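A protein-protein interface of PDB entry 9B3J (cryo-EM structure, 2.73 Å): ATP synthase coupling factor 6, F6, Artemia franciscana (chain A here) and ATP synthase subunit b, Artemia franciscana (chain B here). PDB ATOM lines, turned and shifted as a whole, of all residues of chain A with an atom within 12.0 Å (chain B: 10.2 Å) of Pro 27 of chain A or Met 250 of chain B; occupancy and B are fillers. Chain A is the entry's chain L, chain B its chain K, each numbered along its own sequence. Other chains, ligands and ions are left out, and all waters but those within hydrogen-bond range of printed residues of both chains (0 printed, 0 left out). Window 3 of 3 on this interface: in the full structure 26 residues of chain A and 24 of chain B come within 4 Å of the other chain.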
ATOM      1  N   LYS A  23      20.047  -2.478  40.336  1.00  0.00           N
ATOM      2  CA  LYS A  23      18.705  -2.938  40.001  1.00  0.00           C
ATOM      3  C   LYS A  23      18.342  -2.569  38.565  1.00  0.00           C
ATOM      4  O   LYS A  23      18.776  -1.539  38.052  1.00  0.00           O
ATOM      5  CB  LYS A  23      17.678  -2.351  40.971  1.00  0.00           C
ATOM      6  CG  LYS A  23      17.923  -2.712  42.427  1.00  0.00           C
ATOM      7  CD  LYS A  23      16.887  -2.071  43.337  1.00  0.00           C
ATOM      8  CE  LYS A  23      17.135  -2.428  44.793  1.00  0.00           C
ATOM      9  NZ  LYS A  23      16.126  -1.812  45.698  1.00  0.00           N
ATOM     10  N   ALA A  24      17.545  -3.420  37.922  1.00  0.00           N
ATOM     11  CA  ALA A  24      17.115  -3.191  36.542  1.00  0.00           C
ATOM     12  C   ALA A  24      15.874  -2.297  36.535  1.00  0.00           C
ATOM     13  O   ALA A  24      14.743  -2.730  36.307  1.00  0.00           O
ATOM     14  CB  ALA A  24      16.862  -4.515  35.835  1.00  0.00           C
ATOM     15  N   VAL A  25      16.114  -1.015  36.795  1.00  0.00           N
ATOM     16  CA  VAL A  25      15.043  -0.027  36.827  1.00  0.00           C
ATOM     17  C   VAL A  25      14.646   0.319  35.399  1.00  0.00           C
ATOM     18  O   VAL A  25      15.497   0.668  34.572  1.00  0.00           O
ATOM     19  CB  VAL A  25      15.481   1.226  37.602  1.00  0.00           C
ATOM     20  CG1 VAL A  25      14.351   2.243  37.654  1.00  0.00           C
ATOM     21  CG2 VAL A  25      15.931   0.849  39.005  1.00  0.00           C
ATOM     22  N   ASP A  26      13.354   0.211  35.105  1.00  0.00           N
ATOM     23  CA  ASP A  26      12.864   0.547  33.777  1.00  0.00           C
ATOM     24  C   ASP A  26      12.968   2.053  33.544  1.00  0.00           C
ATOM     25  O   ASP A  26      12.748   2.841  34.469  1.00  0.00           O
ATOM     26  CB  ASP A  26      11.415   0.089  33.607  1.00  0.00           C
ATOM     27  CG  ASP A  26      11.273  -1.419  33.640  1.00  0.00           C
ATOM     28  OD1 ASP A  26      12.307  -2.114  33.720  1.00  0.00           O
ATOM     29  OD2 ASP A  26      10.127  -1.912  33.586  1.00  0.00           O
ATOM     30  N   PRO A  27      13.332   2.480  32.329  1.00  0.00           N
ATOM     31  CA  PRO A  27      13.402   3.924  32.049  1.00  0.00           C
ATOM     32  C   PRO A  27      12.064   4.631  32.144  1.00  0.00           C
ATOM     33  O   PRO A  27      12.027   5.813  32.507  1.00  0.00           O
ATOM     34  CB  PRO A  27      13.967   3.973  30.623  1.00  0.00           C
ATOM     35  CG  PRO A  27      13.588   2.663  30.027  1.00  0.00           C
ATOM     36  CD  PRO A  27      13.667   1.670  31.147  1.00  0.00           C
ATOM     37  N   ILE A  28      10.963   3.945  31.830  1.00  0.00           N
ATOM     38  CA  ILE A  28       9.649   4.577  31.893  1.00  0.00           C
ATOM     39  C   ILE A  28       9.245   4.834  33.337  1.00  0.00           C
ATOM     40  O   ILE A  28       8.708   5.898  33.663  1.00  0.00           O
ATOM     41  CB  ILE A  28       8.611   3.716  31.150  1.00  0.00           C
ATOM     42  CG1 ILE A  28       8.990   3.606  29.675  1.00  0.00           C
ATOM     43  CG2 ILE A  28       7.217   4.310  31.276  1.00  0.00           C
ATOM     44  CD1 ILE A  28       9.091   4.945  28.983  1.00  0.00           C
ATOM     45  N   GLN A  29       9.506   3.871  34.227  1.00  0.00           N
ATOM     46  CA  GLN A  29       9.191   4.059  35.640  1.00  0.00           C
ATOM     47  C   GLN A  29      10.027   5.177  36.253  1.00  0.00           C
ATOM     48  O   GLN A  29       9.512   5.998  37.021  1.00  0.00           O
ATOM     49  CB  GLN A  29       9.404   2.753  36.403  1.00  0.00           C
ATOM     50  CG  GLN A  29       8.504   1.622  35.948  1.00  0.00           C
ATOM     51  CD  GLN A  29       8.655   0.378  36.799  1.00  0.00           C
ATOM     52  OE1 GLN A  29       9.335   0.392  37.825  1.00  0.00           O
ATOM     53  NE2 GLN A  29       8.021  -0.709  36.377  1.00  0.00           N
ATOM     54  N   LYS A  30      11.319   5.226  35.915  1.00  0.00           N
ATOM     55  CA  LYS A  30      12.181   6.290  36.419  1.00  0.00           C
ATOM     56  C   LYS A  30      11.764   7.648  35.869  1.00  0.00           C
ATOM     57  O   LYS A  30      11.788   8.650  36.594  1.00  0.00           O
ATOM     58  CB  LYS A  30      13.638   5.991  36.069  1.00  0.00           C
ATOM     59  CG  LYS A  30      14.637   6.938  36.709  1.00  0.00           C
ATOM     60  CD  LYS A  30      16.063   6.494  36.435  1.00  0.00           C
ATOM     61  CE  LYS A  30      17.065   7.399  37.128  1.00  0.00           C
ATOM     62  NZ  LYS A  30      18.467   6.947  36.906  1.00  0.00           N
ATOM     63  N   LEU A  31      11.370   7.700  34.593  1.00  0.00           N
ATOM     64  CA  LEU A  31      10.883   8.945  34.008  1.00  0.00           C
ATOM     65  C   LEU A  31       9.583   9.394  34.662  1.00  0.00           C
ATOM     66  O   LEU A  31       9.386  10.591  34.903  1.00  0.00           O
ATOM     67  CB  LEU A  31      10.698   8.774  32.500  1.00  0.00           C
ATOM     68  CG  LEU A  31      10.283  10.008  31.701  1.00  0.00           C
ATOM     69  CD1 LEU A  31      11.278  11.139  31.901  1.00  0.00           C
ATOM     70  CD2 LEU A  31      10.161   9.658  30.228  1.00  0.00           C
ATOM     71  N   PHE A  32       8.688   8.448  34.959  1.00  0.00           N
ATOM     72  CA  PHE A  32       7.445   8.779  35.650  1.00  0.00           C
ATOM     73  C   PHE A  32       7.714   9.314  37.051  1.00  0.00           C
ATOM     74  O   PHE A  32       7.076  10.280  37.487  1.00  0.00           O
ATOM     75  CB  PHE A  32       6.537   7.551  35.713  1.00  0.00           C
ATOM     76  CG  PHE A  32       5.469   7.530  34.658  1.00  0.00           C
ATOM     77  CD1 PHE A  32       4.281   8.219  34.844  1.00  0.00           C
ATOM     78  CD2 PHE A  32       5.648   6.818  33.484  1.00  0.00           C
ATOM     79  CE1 PHE A  32       3.293   8.200  33.875  1.00  0.00           C
ATOM     80  CE2 PHE A  32       4.664   6.795  32.511  1.00  0.00           C
ATOM     81  CZ  PHE A  32       3.486   7.486  32.708  1.00  0.00           C
ATOM     82  N   LEU A  33       8.663   8.700  37.765  1.00  0.00           N
ATOM     83  CA  LEU A  33       9.021   9.186  39.096  1.00  0.00           C
ATOM     84  C   LEU A  33       9.651  10.572  39.030  1.00  0.00           C
ATOM     85  O   LEU A  33       9.397  11.417  39.900  1.00  0.00           O
ATOM     86  CB  LEU A  33       9.965   8.200  39.781  1.00  0.00           C
ATOM     87  CG  LEU A  33       9.372   6.852  40.195  1.00  0.00           C
ATOM     88  CD1 LEU A  33      10.407   6.009  40.926  1.00  0.00           C
ATOM     89  CD2 LEU A  33       8.132   7.049  41.051  1.00  0.00           C
ATOM     90  N   ASP A  34      10.477  10.821  38.010  1.00  0.00           N
ATOM     91  CA  ASP A  34      11.079  12.141  37.843  1.00  0.00           C
ATOM     92  C   ASP A  34      10.028  13.200  37.534  1.00  0.00           C
ATOM     93  O   ASP A  34      10.111  14.325  38.038  1.00  0.00           O
ATOM     94  CB  ASP A  34      12.137  12.098  36.742  1.00  0.00           C
ATOM     95  CG  ASP A  34      13.346  11.274  37.131  1.00  0.00           C
ATOM     96  OD1 ASP A  34      13.358  10.732  38.257  1.00  0.00           O
ATOM     97  OD2 ASP A  34      14.283  11.163  36.313  1.00  0.00           O
ATOM     98  N   LYS A  35       9.029  12.857  36.715  1.00  0.00           N
ATOM     99  CA  LYS A  35       7.966  13.811  36.411  1.00  0.00           C
ATOM    100  C   LYS A  35       7.091  14.079  37.629  1.00  0.00           C
ATOM    101  O   LYS A  35       6.625  15.206  37.827  1.00  0.00           O
ATOM    102  CB  LYS A  35       7.120  13.307  35.244  1.00  0.00           C
ATOM    103  CG  LYS A  35       7.860  13.268  33.922  1.00  0.00           C
ATOM    104  CD  LYS A  35       8.550  14.589  33.634  1.00  0.00           C
ATOM    105  CE  LYS A  35       9.326  14.530  32.331  1.00  0.00           C
ATOM    106  NZ  LYS A  35       9.972  15.830  32.005  1.00  0.00           N
ATOM    107  N   ILE A  36       6.852  13.053  38.451  1.00  0.00           N
ATOM    108  CA  ILE A  36       6.085  13.244  39.679  1.00  0.00           C
ATOM    109  C   ILE A  36       6.836  14.149  40.650  1.00  0.00           C
ATOM    110  O   ILE A  36       6.248  15.057  41.255  1.00  0.00           O
ATOM    111  CB  ILE A  36       5.750  11.877  40.303  1.00  0.00           C
ATOM    112  CG1 ILE A  36       4.664  11.183  39.484  1.00  0.00           C
ATOM    113  CG2 ILE A  36       5.311  12.020  41.753  1.00  0.00           C
ATOM    114  CD1 ILE A  36       4.232   9.858  40.049  1.00  0.00           C
ATOM    115  N   VAL B 238       4.579  13.555  29.870  1.00  0.00           N
ATOM    116  CA  VAL B 238       5.215  12.320  29.425  1.00  0.00           C
ATOM    117  C   VAL B 238       5.197  12.237  27.904  1.00  0.00           C
ATOM    118  O   VAL B 238       6.195  11.854  27.278  1.00  0.00           O
ATOM    119  CB  VAL B 238       4.535  11.104  30.086  1.00  0.00           C
ATOM    120  CG1 VAL B 238       4.749   9.831  29.274  1.00  0.00           C
ATOM    121  CG2 VAL B 238       5.071  10.909  31.495  1.00  0.00           C
ATOM    122  N   SER B 241       7.910  14.363  26.964  1.00  0.00           N
ATOM    123  CA  SER B 241       9.193  14.026  27.567  1.00  0.00           C
ATOM    124  C   SER B 241      10.101  13.217  26.652  1.00  0.00           C
ATOM    125  O   SER B 241      11.244  12.941  27.029  1.00  0.00           O
ATOM    126  CB  SER B 241       8.980  13.243  28.865  1.00  0.00           C
ATOM    127  OG  SER B 241       8.389  11.983  28.601  1.00  0.00           O
ATOM    128  N   ILE B 242       9.634  12.831  25.471  1.00  0.00           N
ATOM    129  CA  ILE B 242      10.388  11.916  24.622  1.00  0.00           C
ATOM    130  C   ILE B 242      11.420  12.702  23.822  1.00  0.00           C
ATOM    131  O   ILE B 242      11.078  13.640  23.094  1.00  0.00           O
ATOM    132  CB  ILE B 242       9.453  11.125  23.696  1.00  0.00           C
ATOM    133  CG1 ILE B 242       8.454  10.314  24.524  1.00  0.00           C
ATOM    134  CG2 ILE B 242      10.257  10.213  22.781  1.00  0.00           C
ATOM    135  CD1 ILE B 242       7.484   9.507  23.693  1.00  0.00           C
ATOM    136  N   THR B 243      12.687  12.317  23.959  1.00  0.00           N
ATOM    137  CA  THR B 243      13.796  12.848  23.186  1.00  0.00           C
ATOM    138  C   THR B 243      14.416  11.727  22.358  1.00  0.00           C
ATOM    139  O   THR B 243      14.389  10.565  22.778  1.00  0.00           O
ATOM    140  CB  THR B 243      14.862  13.472  24.099  1.00  0.00           C
ATOM    141  OG1 THR B 243      15.340  12.489  25.023  1.00  0.00           O
ATOM    142  CG2 THR B 243      14.281  14.647  24.869  1.00  0.00           C
ATOM    143  N   PRO B 244      14.944  12.033  21.165  1.00  0.00           N
ATOM    144  CA  PRO B 244      15.489  10.964  20.306  1.00  0.00           C
ATOM    145  C   PRO B 244      16.656  10.200  20.914  1.00  0.00           C
ATOM    146  O   PRO B 244      16.779   8.994  20.669  1.00  0.00           O
ATOM    147  CB  PRO B 244      15.911  11.718  19.036  1.00  0.00           C
ATOM    148  CG  PRO B 244      16.045  13.143  19.454  1.00  0.00           C
ATOM    149  CD  PRO B 244      14.990  13.343  20.493  1.00  0.00           C
ATOM    150  N   GLU B 245      17.514  10.860  21.697  1.00  0.00           N
ATOM    151  CA  GLU B 245      18.616  10.149  22.342  1.00  0.00           C
ATOM    152  C   GLU B 245      18.106   9.172  23.396  1.00  0.00           C
ATOM    153  O   GLU B 245      18.596   8.039  23.493  1.00  0.00           O
ATOM    154  CB  GLU B 245      19.608  11.142  22.954  1.00  0.00           C
ATOM    155  CG  GLU B 245      18.982  12.289  23.737  1.00  0.00           C
ATOM    156  CD  GLU B 245      18.727  13.513  22.880  1.00  0.00           C
ATOM    157  OE1 GLU B 245      19.162  13.519  21.709  1.00  0.00           O
ATOM    158  OE2 GLU B 245      18.091  14.466  23.376  1.00  0.00           O
ATOM    159  N   GLN B 246      17.104   9.581  24.179  1.00  0.00           N
ATOM    160  CA  GLN B 246      16.509   8.670  25.147  1.00  0.00           C
ATOM    161  C   GLN B 246      15.696   7.583  24.458  1.00  0.00           C
ATOM    162  O   GLN B 246      15.596   6.466  24.974  1.00  0.00           O
ATOM    163  CB  GLN B 246      15.641   9.445  26.138  1.00  0.00           C
ATOM    164  CG  GLN B 246      15.288   8.681  27.404  1.00  0.00           C
ATOM    165  CD  GLN B 246      14.633   9.560  28.454  1.00  0.00           C
ATOM    166  OE1 GLN B 246      14.473  10.765  28.259  1.00  0.00           O
ATOM    167  NE2 GLN B 246      14.253   8.960  29.576  1.00  0.00           N
ATOM    168  N   GLU B 247      15.120   7.888  23.291  1.00  0.00           N
ATOM    169  CA  GLU B 247      14.433   6.864  22.510  1.00  0.00           C
ATOM    170  C   GLU B 247      15.405   5.797  22.018  1.00  0.00           C
ATOM    171  O   GLU B 247      15.096   4.601  22.059  1.00  0.00           O
ATOM    172  CB  GLU B 247      13.703   7.507  21.331  1.00  0.00           C
ATOM    173  CG  GLU B 247      12.942   6.521  20.462  1.00  0.00           C
ATOM    174  CD  GLU B 247      12.292   7.180  19.264  1.00  0.00           C
ATOM    175  OE1 GLU B 247      12.407   8.417  19.129  1.00  0.00           O
ATOM    176  OE2 GLU B 247      11.666   6.463  18.455  1.00  0.00           O
ATOM    177  N   ARG B 248      16.587   6.215  21.557  1.00  0.00           N
ATOM    178  CA  ARG B 248      17.611   5.253  21.156  1.00  0.00           C
ATOM    179  C   ARG B 248      18.110   4.445  22.347  1.00  0.00           C
ATOM    180  O   ARG B 248      18.379   3.243  22.220  1.00  0.00           O
ATOM    181  CB  ARG B 248      18.773   5.973  20.477  1.00  0.00           C
ATOM    182  CG  ARG B 248      18.418   6.615  19.150  1.00  0.00           C
ATOM    183  CD  ARG B 248      19.576   7.438  18.611  1.00  0.00           C
ATOM    184  NE  ARG B 248      19.221   8.132  17.379  1.00  0.00           N
ATOM    185  CZ  ARG B 248      20.040   8.923  16.701  1.00  0.00           C
ATOM    186  NH1 ARG B 248      21.280   9.145  17.107  1.00  0.00           N
ATOM    187  NH2 ARG B 248      19.606   9.509  15.589  1.00  0.00           N
ATOM    188  N   LEU B 249      18.247   5.091  23.510  1.00  0.00           N
ATOM    189  CA  LEU B 249      18.658   4.373  24.715  1.00  0.00           C
ATOM    190  C   LEU B 249      17.616   3.343  25.138  1.00  0.00           C
ATOM    191  O   LEU B 249      17.964   2.227  25.546  1.00  0.00           O
ATOM    192  CB  LEU B 249      18.923   5.362  25.850  1.00  0.00           C
ATOM    193  CG  LEU B 249      20.197   6.204  25.751  1.00  0.00           C
ATOM    194  CD1 LEU B 249      20.278   7.192  26.905  1.00  0.00           C
ATOM    195  CD2 LEU B 249      21.431   5.315  25.718  1.00  0.00           C
ATOM    196  N   MET B 250      16.332   3.696  25.044  1.00  0.00           N
ATOM    197  CA  MET B 250      15.274   2.757  25.404  1.00  0.00           C
ATOM    198  C   MET B 250      15.183   1.613  24.401  1.00  0.00           C
ATOM    199  O   MET B 250      14.918   0.469  24.785  1.00  0.00           O
ATOM    200  CB  MET B 250      13.935   3.483  25.514  1.00  0.00           C
ATOM    201  CG  MET B 250      13.816   4.363  26.746  1.00  0.00           C
ATOM    202  SD  MET B 250      12.198   5.135  26.911  1.00  0.00           S
ATOM    203  CE  MET B 250      12.106   6.049  25.375  1.00  0.00           C
ATOM    204  N   LEU B 251      15.397   1.902  23.114  1.00  0.00           N
ATOM    205  CA  LEU B 251      15.415   0.843  22.109  1.00  0.00           C
ATOM    206  C   LEU B 251      16.584  -0.109  22.329  1.00  0.00           C
ATOM    207  O   LEU B 251      16.433  -1.329  22.188  1.00  0.00           O
ATOM    208  CB  LEU B 251      15.472   1.445  20.708  1.00  0.00           C
ATOM    209  CG  LEU B 251      14.159   1.475  19.925  1.00  0.00           C
ATOM    210  CD1 LEU B 251      13.121   2.331  20.631  1.00  0.00           C
ATOM    211  CD2 LEU B 251      14.394   1.970  18.508  1.00  0.00           C
ATOM    212  N   SER B 252      17.756   0.431  22.680  1.00  0.00           N
ATOM    213  CA  SER B 252      18.906  -0.416  22.979  1.00  0.00           C
ATOM    214  C   SER B 252      18.669  -1.251  24.230  1.00  0.00           C
ATOM    215  O   SER B 252      19.083  -2.415  24.295  1.00  0.00           O
ATOM    216  CB  SER B 252      20.158   0.443  23.140  1.00  0.00           C
ATOM    217  OG  SER B 252      20.019   1.342  24.226  1.00  0.00           O
ATOM    218  N   LYS B 253      18.001  -0.676  25.235  1.00  0.00           N
ATOM    219  CA  LYS B 253      17.683  -1.431  26.443  1.00  0.00           C
ATOM    220  C   LYS B 253      16.671  -2.536  26.158  1.00  0.00           C
ATOM    221  O   LYS B 253      16.773  -3.634  26.715  1.00  0.00           O
ATOM    222  CB  LYS B 253      17.166  -0.488  27.528  1.00  0.00           C
ATOM    223  CG  LYS B 253      16.999  -1.147  28.887  1.00  0.00           C
ATOM    224  CD  LYS B 253      16.724  -0.121  29.973  1.00  0.00           C
ATOM    225  CE  LYS B 253      16.657  -0.775  31.343  1.00  0.00           C
ATOM    226  NZ  LYS B 253      16.492   0.228  32.430  1.00  0.00           N
ATOM    227  N   CYS B 254      15.687  -2.263  25.296  1.00  0.00           N
ATOM    228  CA  CYS B 254      14.725  -3.290  24.908  1.00  0.00           C
ATOM    229  C   CYS B 254      15.393  -4.411  24.122  1.00  0.00           C
ATOM    230  O   CYS B 254      15.055  -5.587  24.301  1.00  0.00           O
ATOM    231  CB  CYS B 254      13.589  -2.671  24.096  1.00  0.00           C
ATOM    232  SG  CYS B 254      12.458  -1.641  25.057  1.00  0.00           S
ATOM    233  N   ILE B 255      16.339  -4.064  23.244  1.00  0.00           N
ATOM    234  CA  ILE B 255      17.088  -5.079  22.506  1.00  0.00           C
ATOM    235  C   ILE B 255      17.939  -5.916  23.456  1.00  0.00           C
ATOM    236  O   ILE B 255      18.027  -7.142  23.313  1.00  0.00           O
ATOM    237  CB  ILE B 255      17.930  -4.409  21.404  1.00  0.00           C
ATOM    238  CG1 ILE B 255      17.020  -3.899  20.286  1.00  0.00           C
ATOM    239  CG2 ILE B 255      18.967  -5.365  20.830  1.00  0.00           C
ATOM    240  CD1 ILE B 255      17.755  -3.194  19.169  1.00  0.00           C
ATOM    241  N   SER B 256      18.559  -5.273  24.451  1.00  0.00           N
ATOM    242  CA  SER B 256      19.345  -6.004  25.441  1.00  0.00           C
ATOM    243  C   SER B 256      18.471  -6.930  26.281  1.00  0.00           C
ATOM    244  O   SER B 256      18.879  -8.049  26.607  1.00  0.00           O
ATOM    245  CB  SER B 256      20.098  -5.025  26.341  1.00  0.00           C
ATOM    246  OG  SER B 256      19.198  -4.297  27.156  1.00  0.00           O
ATOM    247  N   ASP B 257      17.267  -6.478  26.642  1.00  0.00           N
ATOM    248  CA  ASP B 257      16.341  -7.334  27.382  1.00  0.00           C
ATOM    249  C   ASP B 257      15.863  -8.504  26.531  1.00  0.00           C
ATOM    250  O   ASP B 257      15.709  -9.624  27.034  1.00  0.00           O
ATOM    251  CB  ASP B 257      15.152  -6.514  27.879  1.00  0.00           C
ATOM    252  CG  ASP B 257      15.546  -5.480  28.912  1.00  0.00           C
ATOM    253  OD1 ASP B 257      16.538  -5.711  29.634  1.00  0.00           O
ATOM    254  OD2 ASP B 257      14.865  -4.438  29.001  1.00  0.00           O
ATOM    255  N   LEU B 258      15.619  -8.262  25.240  1.00  0.00           N
ATOM    256  CA  LEU B 258      15.239  -9.341  24.333  1.00  0.00           C
ATOM    257  C   LEU B 258      16.371 -10.347  24.167  1.00  0.00           C
ATOM    258  O   LEU B 258      16.132 -11.558  24.105  1.00  0.00           O
ATOM    259  CB  LEU B 258      14.826  -8.758  22.981  1.00  0.00           C
ATOM    260  CG  LEU B 258      14.369  -9.732  21.896  1.00  0.00           C
ATOM    261  CD1 LEU B 258      13.182 -10.550  22.370  1.00  0.00           C
ATOM    262  CD2 LEU B 258      14.024  -8.975  20.627  1.00  0.00           C
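The backbone carbonyl oxygen (O) of Val 25 of chain A is in hydrogen-bond range of the side-chain amino group (NZ) of Lys 253 of chain B, at 2.4 Å.
OG of Ser 241 of chain B is in hydrogen-bond range of O of Val 238 of chain B (2.6 Å).
The side-chain sulfur (SG) of Cys 254 of chain B sits at hydrogen-bond distance from the backbone carbonyl oxygen (O) of Met 250 of chain B, at 3.3 Å.
The backbone carbonyl oxygen of Lys 253 of chain B sits at hydrogen-bond distance from the side-chain hydroxyl of Ser 256 of chain B (2.6 Å).
Lys 253 of chain B touches Asp 26 of chain A (NZ to CA, 3.9 Å).
Pro 27 of chain A touches Met 250 of chain B (CG to CG, 3.7 Å).
NZ of Lys 253 of chain B touches CD of Pro 27 of chain A (3.4 Å).
CD1 of Ile 28 of chain A touches SD of Met 250 of chain B, at 3.7 Å.
Leu 31 of chain A touches Ser 241 of chain B.
Val 238 of chain B touches Phe 32 of chain A.
CB of Ser 241 of chain B touches CE of Lys 35 of chain A, 3.7 Å away.
Of chain B, only Met 250 and Lys 253 come within 4 Å of Pro 27 of chain A.
Of the printed residues of chain A, Met 250 of chain B touches Pro 27 (3.7 Å) and Ile 28 (3.7 Å).
Of the printed residues of chain B, Ile 28 of chain A touches Met 250 (3.7 Å).
Of chain B, only Ser 241 comes within 4 Å of Leu 31 of chain A.
No residue of chain A comes within 4 Å of Gln 246 of chain B.
No residue of chain A comes within 4 Å of Glu 247 of chain B.
No residue of chain A comes within 4 Å of Leu 249 of chain B.
No residue of chain A comes within 4 Å of Leu 251 of chain B.
Ser 252 of chain B touches none of the printed residues of chain A.
No residue of chain A comes within 4 Å of Cys 254 of chain B.
Of the printed residues of chain A, Val 238 of chain B touches Phe 32.
Of the printed residues of chain B, Phe 32 of chain A touches Val 238.
Of the printed residues of chain B, Lys 35 of chain A touches Ser 241.
Of the printed residues of chain B, Val 25 of chain A touches Lys 253 (2.4 Å).
Leu 258 of chain B touches none of the printed residues of chain A.
The nearest printed residue of chain A that does not touch Val 238 of chain B is Lys 35 of chain A (4.4 Å).
Hydrophobic or aromatic side chains of chain A that line the printed part of chain B: Pro 27, Ile 28, Leu 31 and Phe 32.
Of the 19 printed residues of chain B, 4 touch a printed residue of chain A.
Hydrophobic or aromatic side chains of chain B that line the printed part of chain A: Val 238 and Met 250.
Among the printed residues, 8 pairs touch across the chains.
Among the printed residues, no Asp or Glu carboxylate lies within 4 Å of a Lys or Arg side-chain nitrogen of the other chain.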
